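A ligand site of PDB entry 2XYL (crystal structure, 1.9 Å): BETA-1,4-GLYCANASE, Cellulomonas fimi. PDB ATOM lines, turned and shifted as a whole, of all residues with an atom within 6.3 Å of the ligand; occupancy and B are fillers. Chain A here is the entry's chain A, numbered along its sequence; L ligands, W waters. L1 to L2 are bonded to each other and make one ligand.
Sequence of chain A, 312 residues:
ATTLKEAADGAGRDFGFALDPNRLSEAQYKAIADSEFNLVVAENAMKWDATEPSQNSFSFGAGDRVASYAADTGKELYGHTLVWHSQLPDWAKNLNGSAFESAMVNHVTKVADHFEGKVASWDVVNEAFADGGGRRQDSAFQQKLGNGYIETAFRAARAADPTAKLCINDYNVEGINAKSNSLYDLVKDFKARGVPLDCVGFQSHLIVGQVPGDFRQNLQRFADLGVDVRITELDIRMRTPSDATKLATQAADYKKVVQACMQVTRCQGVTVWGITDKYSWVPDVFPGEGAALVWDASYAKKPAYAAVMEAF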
ATOM      1  N   GLU A  43     -28.673  34.659 -29.489  1.00  0.00           N
ATOM      2  CA  GLU A  43     -29.534  33.954 -28.551  1.00  0.00           C
ATOM      3  C   GLU A  43     -29.486  32.450 -28.831  1.00  0.00           C
ATOM      4  O   GLU A  43     -29.470  31.640 -27.897  1.00  0.00           O
ATOM      5  CB  GLU A  43     -30.987  34.451 -28.643  1.00  0.00           C
ATOM      6  CG  GLU A  43     -31.927  33.789 -27.634  1.00  0.00           C
ATOM      7  CD  GLU A  43     -33.391  34.186 -27.809  1.00  0.00           C
ATOM      8  OE1 GLU A  43     -33.817  34.473 -28.953  1.00  0.00           O
ATOM      9  OE2 GLU A  43     -34.131  34.180 -26.797  1.00  0.00           O
ATOM     10  N   ASN A  44     -29.422  32.086 -30.104  1.00  0.00           N
ATOM     11  CA  ASN A  44     -29.389  30.677 -30.496  1.00  0.00           C
ATOM     12  C   ASN A  44     -28.538  30.391 -31.723  1.00  0.00           C
ATOM     13  O   ASN A  44     -28.076  29.268 -31.907  1.00  0.00           O
ATOM     14  CB  ASN A  44     -30.814  30.162 -30.775  1.00  0.00           C
ATOM     15  CG  ASN A  44     -31.671  30.104 -29.529  1.00  0.00           C
ATOM     16  OD1 ASN A  44     -31.493  29.239 -28.669  1.00  0.00           O
ATOM     17  ND2 ASN A  44     -32.621  31.019 -29.422  1.00  0.00           N
ATOM     18  N   LYS A  47     -25.084  28.282 -31.379  1.00  0.00           N
ATOM     19  CA  LYS A  47     -25.055  27.037 -30.619  1.00  0.00           C
ATOM     20  C   LYS A  47     -24.723  25.838 -31.511  1.00  0.00           C
ATOM     21  O   LYS A  47     -24.687  25.957 -32.742  1.00  0.00           O
ATOM     22  CB  LYS A  47     -26.384  26.822 -29.876  1.00  0.00           C
ATOM     23  CG  LYS A  47     -26.623  27.844 -28.779  1.00  0.00           C
ATOM     24  CD  LYS A  47     -28.011  27.750 -28.175  1.00  0.00           C
ATOM     25  CE  LYS A  47     -28.193  28.810 -27.103  1.00  0.00           C
ATOM     26  NZ  LYS A  47     -29.596  28.900 -26.613  1.00  0.00           N
ATOM     27  N   HIS A  80     -21.577  32.854 -28.113  1.00  0.00           N
ATOM     28  CA  HIS A  80     -22.287  32.031 -27.154  1.00  0.00           C
ATOM     29  C   HIS A  80     -22.190  30.520 -27.323  1.00  0.00           C
ATOM     30  O   HIS A  80     -22.707  29.932 -28.266  1.00  0.00           O
ATOM     31  CB  HIS A  80     -23.746  32.453 -27.011  1.00  0.00           C
ATOM     32  CG  HIS A  80     -24.464  31.752 -25.900  1.00  0.00           C
ATOM     33  ND1 HIS A  80     -23.900  31.574 -24.657  1.00  0.00           N
ATOM     34  CD2 HIS A  80     -25.670  31.141 -25.857  1.00  0.00           C
ATOM     35  CE1 HIS A  80     -24.735  30.890 -23.891  1.00  0.00           C
ATOM     36  NE2 HIS A  80     -25.818  30.617 -24.592  1.00  0.00           N
ATOM     37  N   THR A  81     -21.518  29.957 -26.330  1.00  0.00           N
ATOM     38  CA  THR A  81     -21.234  28.540 -26.152  1.00  0.00           C
ATOM     39  C   THR A  81     -20.871  27.569 -27.273  1.00  0.00           C
ATOM     40  O   THR A  81     -21.650  27.304 -28.195  1.00  0.00           O
ATOM     41  CB  THR A  81     -22.236  27.900 -25.186  1.00  0.00           C
ATOM     42  OG1 THR A  81     -21.641  26.747 -24.587  1.00  0.00           O
ATOM     43  CG2 THR A  81     -23.527  27.511 -25.898  1.00  0.00           C
ATOM     44  N   TRP A  84     -21.935  22.620 -24.707  1.00  0.00           N
ATOM     45  CA  TRP A  84     -23.107  22.703 -23.838  1.00  0.00           C
ATOM     46  C   TRP A  84     -23.921  21.422 -23.969  1.00  0.00           C
ATOM     47  O   TRP A  84     -24.150  20.942 -25.079  1.00  0.00           O
ATOM     48  CB  TRP A  84     -23.955  23.908 -24.247  1.00  0.00           C
ATOM     49  CG  TRP A  84     -25.052  24.256 -23.296  1.00  0.00           C
ATOM     50  CD1 TRP A  84     -25.067  24.049 -21.949  1.00  0.00           C
ATOM     51  CD2 TRP A  84     -26.284  24.924 -23.606  1.00  0.00           C
ATOM     52  NE1 TRP A  84     -26.234  24.530 -21.408  1.00  0.00           N
ATOM     53  CE2 TRP A  84     -27.001  25.075 -22.401  1.00  0.00           C
ATOM     54  CE3 TRP A  84     -26.853  25.398 -24.800  1.00  0.00           C
ATOM     55  CZ2 TRP A  84     -28.256  25.687 -22.342  1.00  0.00           C
ATOM     56  CZ3 TRP A  84     -28.101  26.005 -24.741  1.00  0.00           C
ATOM     57  CH2 TRP A  84     -28.791  26.139 -23.524  1.00  0.00           C
ATOM     58  N   SER A  86     -27.084  21.027 -23.433  1.00  0.00           N
ATOM     59  CA  SER A  86     -28.398  21.293 -24.028  1.00  0.00           C
ATOM     60  C   SER A  86     -28.246  21.738 -25.484  1.00  0.00           C
ATOM     61  O   SER A  86     -27.203  22.250 -25.881  1.00  0.00           O
ATOM     62  CB  SER A  86     -29.147  22.351 -23.212  1.00  0.00           C
ATOM     63  OG  SER A  86     -30.487  22.489 -23.652  1.00  0.00           O
ATOM     64  N   GLN A  87     -29.309  21.538 -26.264  1.00  0.00           N
ATOM     65  CA  GLN A  87     -29.327  21.877 -27.683  1.00  0.00           C
ATOM     66  C   GLN A  87     -28.151  21.246 -28.427  1.00  0.00           C
ATOM     67  O   GLN A  87     -27.437  21.912 -29.179  1.00  0.00           O
ATOM     68  CB  GLN A  87     -29.391  23.396 -27.896  1.00  0.00           C
ATOM     69  CG  GLN A  87     -30.768  23.967 -27.633  1.00  0.00           C
ATOM     70  CD  GLN A  87     -30.855  25.448 -27.943  1.00  0.00           C
ATOM     71  OE1 GLN A  87     -31.015  25.843 -29.097  1.00  0.00           O
ATOM     72  NE2 GLN A  87     -30.780  26.271 -26.907  1.00  0.00           N
ATOM     73  N   ASP A 123     -18.044  31.604 -24.791  1.00  0.00           N
ATOM     74  CA  ASP A 123     -18.528  30.806 -23.672  1.00  0.00           C
ATOM     75  C   ASP A 123     -18.052  29.436 -24.126  1.00  0.00           C
ATOM     76  O   ASP A 123     -18.746  28.758 -24.875  1.00  0.00           O
ATOM     77  CB  ASP A 123     -20.060  30.825 -23.582  1.00  0.00           C
ATOM     78  CG  ASP A 123     -20.595  31.960 -22.746  1.00  0.00           C
ATOM     79  OD1 ASP A 123     -19.844  32.533 -21.930  1.00  0.00           O
ATOM     80  OD2 ASP A 123     -21.796  32.277 -22.887  1.00  0.00           O
ATOM     81  N   ASN A 126     -20.442  25.852 -21.035  1.00  0.00           N
ATOM     82  CA  ASN A 126     -21.621  26.425 -20.410  1.00  0.00           C
ATOM     83  C   ASN A 126     -22.349  25.386 -19.554  1.00  0.00           C
ATOM     84  O   ASN A 126     -22.560  24.247 -19.983  1.00  0.00           O
ATOM     85  CB  ASN A 126     -22.565  26.952 -21.502  1.00  0.00           C
ATOM     86  CG  ASN A 126     -23.748  27.720 -20.952  1.00  0.00           C
ATOM     87  OD1 ASN A 126     -23.575  28.696 -20.218  1.00  0.00           O
ATOM     88  ND2 ASN A 126     -24.944  27.320 -21.346  1.00  0.00           N
ATOM     89  N   GLU A 127     -22.655  25.764 -18.309  1.00  0.00           N
ATOM     90  CA  GLU A 127     -23.384  24.920 -17.362  1.00  0.00           C
ATOM     91  C   GLU A 127     -22.806  23.518 -17.131  1.00  0.00           C
ATOM     92  O   GLU A 127     -23.502  22.512 -17.306  1.00  0.00           O
ATOM     93  CB  GLU A 127     -24.848  24.839 -17.793  1.00  0.00           C
ATOM     94  CG  GLU A 127     -25.486  26.215 -17.941  1.00  0.00           C
ATOM     95  CD  GLU A 127     -26.861  26.183 -18.561  1.00  0.00           C
ATOM     96  OE1 GLU A 127     -27.440  25.082 -18.727  1.00  0.00           O
ATOM     97  OE2 GLU A 127     -27.370  27.271 -18.884  1.00  0.00           O
ATOM     98  N   ASN A 169     -19.269  29.642 -18.381  1.00  0.00           N
ATOM     99  CA  ASN A 169     -20.547  30.246 -18.003  1.00  0.00           C
ATOM    100  C   ASN A 169     -21.436  29.315 -17.185  1.00  0.00           C
ATOM    101  O   ASN A 169     -21.399  28.099 -17.365  1.00  0.00           O
ATOM    102  CB  ASN A 169     -21.260  30.681 -19.283  1.00  0.00           C
ATOM    103  CG  ASN A 169     -22.355  31.699 -19.036  1.00  0.00           C
ATOM    104  OD1 ASN A 169     -22.167  32.662 -18.303  1.00  0.00           O
ATOM    105  ND2 ASN A 169     -23.513  31.489 -19.659  1.00  0.00           N
ATOM    106  N   GLN A 203     -24.774  33.925 -15.338  1.00  0.00           N
ATOM    107  CA  GLN A 203     -26.042  34.050 -16.037  1.00  0.00           C
ATOM    108  C   GLN A 203     -26.999  35.075 -15.443  1.00  0.00           C
ATOM    109  O   GLN A 203     -27.488  35.958 -16.141  1.00  0.00           O
ATOM    110  CB  GLN A 203     -26.715  32.687 -16.190  1.00  0.00           C
ATOM    111  CG  GLN A 203     -25.935  31.745 -17.099  1.00  0.00           C
ATOM    112  CD  GLN A 203     -26.708  30.508 -17.510  1.00  0.00           C
ATOM    113  OE1 GLN A 203     -27.922  30.449 -17.393  1.00  0.00           O
ATOM    114  NE2 GLN A 203     -25.985  29.514 -18.003  1.00  0.00           N
ATOM    115  N   HIS A 205     -30.117  34.604 -13.968  1.00  0.00           N
ATOM    116  CA  HIS A 205     -31.534  34.390 -14.269  1.00  0.00           C
ATOM    117  C   HIS A 205     -32.193  34.417 -12.895  1.00  0.00           C
ATOM    118  O   HIS A 205     -32.456  33.375 -12.285  1.00  0.00           O
ATOM    119  CB  HIS A 205     -31.762  33.043 -14.964  1.00  0.00           C
ATOM    120  CG  HIS A 205     -31.349  33.024 -16.402  1.00  0.00           C
ATOM    121  ND1 HIS A 205     -31.919  33.839 -17.355  1.00  0.00           N
ATOM    122  CD2 HIS A 205     -30.417  32.278 -17.057  1.00  0.00           C
ATOM    123  CE1 HIS A 205     -31.361  33.596 -18.537  1.00  0.00           C
ATOM    124  NE2 HIS A 205     -30.449  32.658 -18.378  1.00  0.00           N
ATOM    125  N   GLU A 233     -26.583  36.555 -18.848  1.00  0.00           N
ATOM    126  CA  GLU A 233     -27.951  36.388 -19.327  1.00  0.00           C
ATOM    127  C   GLU A 233     -28.993  36.920 -18.373  1.00  0.00           C
ATOM    128  O   GLU A 233     -29.964  36.234 -18.039  1.00  0.00           O
ATOM    129  CB  GLU A 233     -28.180  34.901 -19.589  1.00  0.00           C
ATOM    130  CG  GLU A 233     -27.047  34.220 -20.309  1.00  0.00           C
ATOM    131  CD  GLU A 233     -27.256  32.721 -20.459  1.00  0.00           C
ATOM    132  OE1 GLU A 233     -28.562  32.224 -20.798  1.00  0.00           O
ATOM    133  OE2 GLU A 233     -26.276  31.981 -20.288  1.00  0.00           O
ATOM    134  N   TRP A 273     -30.776  39.072 -21.344  1.00  0.00           N
ATOM    135  CA  TRP A 273     -31.202  38.039 -22.266  1.00  0.00           C
ATOM    136  C   TRP A 273     -32.436  38.405 -23.100  1.00  0.00           C
ATOM    137  O   TRP A 273     -33.497  37.792 -22.974  1.00  0.00           O
ATOM    138  CB  TRP A 273     -31.386  36.703 -21.552  1.00  0.00           C
ATOM    139  CG  TRP A 273     -31.119  35.537 -22.451  1.00  0.00           C
ATOM    140  CD1 TRP A 273     -32.008  34.559 -22.802  1.00  0.00           C
ATOM    141  CD2 TRP A 273     -29.910  35.260 -23.149  1.00  0.00           C
ATOM    142  NE1 TRP A 273     -31.418  33.687 -23.694  1.00  0.00           N
ATOM    143  CE2 TRP A 273     -30.128  34.096 -23.918  1.00  0.00           C
ATOM    144  CE3 TRP A 273     -28.656  35.881 -23.209  1.00  0.00           C
ATOM    145  CZ2 TRP A 273     -29.137  33.545 -24.740  1.00  0.00           C
ATOM    146  CZ3 TRP A 273     -27.668  35.327 -24.022  1.00  0.00           C
ATOM    147  CH2 TRP A 273     -27.919  34.169 -24.776  1.00  0.00           C
ATOM    148  N   TRP A 281     -37.697  34.319 -23.300  1.00  0.00           N
ATOM    149  CA  TRP A 281     -37.771  32.859 -23.202  1.00  0.00           C
ATOM    150  C   TRP A 281     -38.412  32.362 -21.911  1.00  0.00           C
ATOM    151  O   TRP A 281     -38.834  31.204 -21.824  1.00  0.00           O
ATOM    152  CB  TRP A 281     -36.362  32.258 -23.314  1.00  0.00           C
ATOM    153  CG  TRP A 281     -35.542  32.388 -22.033  1.00  0.00           C
ATOM    154  CD1 TRP A 281     -35.291  33.532 -21.328  1.00  0.00           C
ATOM    155  CD2 TRP A 281     -34.911  31.318 -21.308  1.00  0.00           C
ATOM    156  NE1 TRP A 281     -34.551  33.243 -20.208  1.00  0.00           N
ATOM    157  CE2 TRP A 281     -34.300  31.900 -20.177  1.00  0.00           C
ATOM    158  CE3 TRP A 281     -34.799  29.946 -21.512  1.00  0.00           C
ATOM    159  CZ2 TRP A 281     -33.593  31.137 -19.245  1.00  0.00           C
ATOM    160  CZ3 TRP A 281     -34.092  29.183 -20.580  1.00  0.00           C
ATOM    161  CH2 TRP A 281     -33.501  29.788 -19.457  1.00  0.00           C
ATOM    162  N   VAL A 285     -40.289  28.409 -20.410  1.00  0.00           N
ATOM    163  CA  VAL A 285     -39.520  27.567 -19.511  1.00  0.00           C
ATOM    164  C   VAL A 285     -40.083  27.596 -18.088  1.00  0.00           C
ATOM    165  O   VAL A 285     -40.188  26.567 -17.440  1.00  0.00           O
ATOM    166  CB  VAL A 285     -38.031  28.012 -19.480  1.00  0.00           C
ATOM    167  CG1 VAL A 285     -37.241  27.205 -18.476  1.00  0.00           C
ATOM    168  CG2 VAL A 285     -37.419  27.871 -20.864  1.00  0.00           C
HETATM  169  C1  LIG L   1     -28.792  30.837 -20.542  1.00  0.00           C
HETATM  170  C2  LIG L   1     -28.247  29.938 -21.687  1.00  0.00           C
HETATM  171  C3  LIG L   1     -28.895  30.282 -23.036  1.00  0.00           C
HETATM  172  C4  LIG L   1     -30.399  30.163 -22.878  1.00  0.00           C
HETATM  173  C5  LIG L   1     -30.838  31.014 -21.688  1.00  0.00           C
HETATM  174  O1  LIG L   1     -28.459  29.390 -24.055  1.00  0.00           O
HETATM  175  O2  LIG L   1     -31.053  30.646 -24.059  1.00  0.00           O
HETATM  176  O3  LIG L   1     -30.187  30.557 -20.499  1.00  0.00           O
HETATM  177  F1  LIG L   1     -26.854  29.941 -21.730  1.00  0.00           F
HETATM  178  C1  LG2 L   2     -32.213  29.968 -24.410  1.00  0.00           C
HETATM  179  C2  LG2 L   2     -32.908  30.722 -25.540  1.00  0.00           C
HETATM  180  C3  LG2 L   2     -34.123  29.986 -26.080  1.00  0.00           C
HETATM  181  C4  LG2 L   2     -33.726  28.566 -26.431  1.00  0.00           C
HETATM  182  C5  LG2 L   2     -33.103  27.879 -25.232  1.00  0.00           C
HETATM  183  O1  LG2 L   2     -33.269  31.996 -25.099  1.00  0.00           O
HETATM  184  O2  LG2 L   2     -34.574  30.656 -27.238  1.00  0.00           O
HETATM  185  O3  LG2 L   2     -34.869  27.834 -26.841  1.00  0.00           O
HETATM  186  O4  LG2 L   2     -31.948  28.626 -24.792  1.00  0.00           O
HETATM  187  O   HOH W   1     -37.345  31.207 -26.488  1.00  0.00           O
HETATM  188  O   HOH W   2     -36.775  27.640 -24.518  1.00  0.00           O
HETATM  189  O   HOH W   3     -31.727  24.911 -24.602  1.00  0.00           O
HETATM  190  O   HOH W   4     -30.136  27.525 -19.752  1.00  0.00           O
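An oxygen (O4) of LG2 L2 lies close to the side-chain amide nitrogen (NE2) of Gln 87 (3.4 Å).
O1 of LIG L1 sits at hydrogen-bond distance from NZ of Lys 47, 2.8 Å away.
O1 of LIG L1 lies within hydrogen-bond range of NE2 of His 80, 3.0 Å away.
ND2 of Asn 44 is in hydrogen-bond range of O2 of LG2 L2 (3.0 Å).
The side-chain carboxylate (OE1) of Glu 233 is bonded to a carbon (C1) of LIG L1 (1.4 Å).
OE2 of Glu 43 lies within hydrogen-bond range of O1 of LG2 L2, 2.9 Å away.
An oxygen (O1) of LG2 L2 sits at hydrogen-bond distance from the indole nitrogen of Trp 273 (2.9 Å).
An oxygen (O3) of LIG L1 is in hydrogen-bond range of a ring nitrogen (NE2) of His 205, at 3.0 Å.
OD2 of Asp 123 lies within hydrogen-bond range of ND1 of His 80 (2.8 Å).
The backbone carbonyl oxygen (O) of Asn 169 lies within hydrogen-bond range of the backbone NH (N) of Glu 127, 2.8 Å away.
O of Glu 43 lies within hydrogen-bond range of NZ of Lys 47, at 3.0 Å.
ND2 of Asn 126 sits close to NE1 of Trp 84.
The side-chain carboxylate of Glu 127 lies within hydrogen-bond range of the side-chain amide nitrogen of Gln 203, at 2.8 Å.
OE1 of Gln 87 lies close to OD1 of Asn 44, at 3.5 Å.
NZ of Lys 47 lies within hydrogen-bond range of OD1 of Asn 44 (2.8 Å).
A ring nitrogen (NE2) of His 205 is in hydrogen-bond range of the side-chain carboxylate of Glu 233, 3.1 Å away.
The side-chain amide nitrogen of Asn 126 sits close to a fluorine (F1) of LIG L1 (3.3 Å).
CH2 of Trp 84 touches O1 of LIG L1 (3.3 Å).
Glu 127 touches the ligand.
OE1 of Gln 203 touches C1 of LIG L1 (3.3 Å).
CH2 of Trp 281 touches O3 of LIG L1 (3.6 Å).
Hydrophobic or aromatic side chains that line the ligand: His 80, Trp 84, His 205, Trp 273 and Trp 281.
13 residues have an atom within 4 Å of the ligand: Glu 43, Asn 44, Lys 47, His 80, Trp 84, Gln 87, Asn 126, Glu 127, Gln 203, His 205, Glu 233, Trp 273 and Trp 281.
The nearest printed residue that does not touch the ligand is Asn 169 (4.2 Å).
Water W4 bridges OE2 of Glu 127 and O3 of LIG L1.
Water W3 bridges the side-chain amide nitrogen of Gln 87 and the side-chain hydroxyl of Ser 86.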
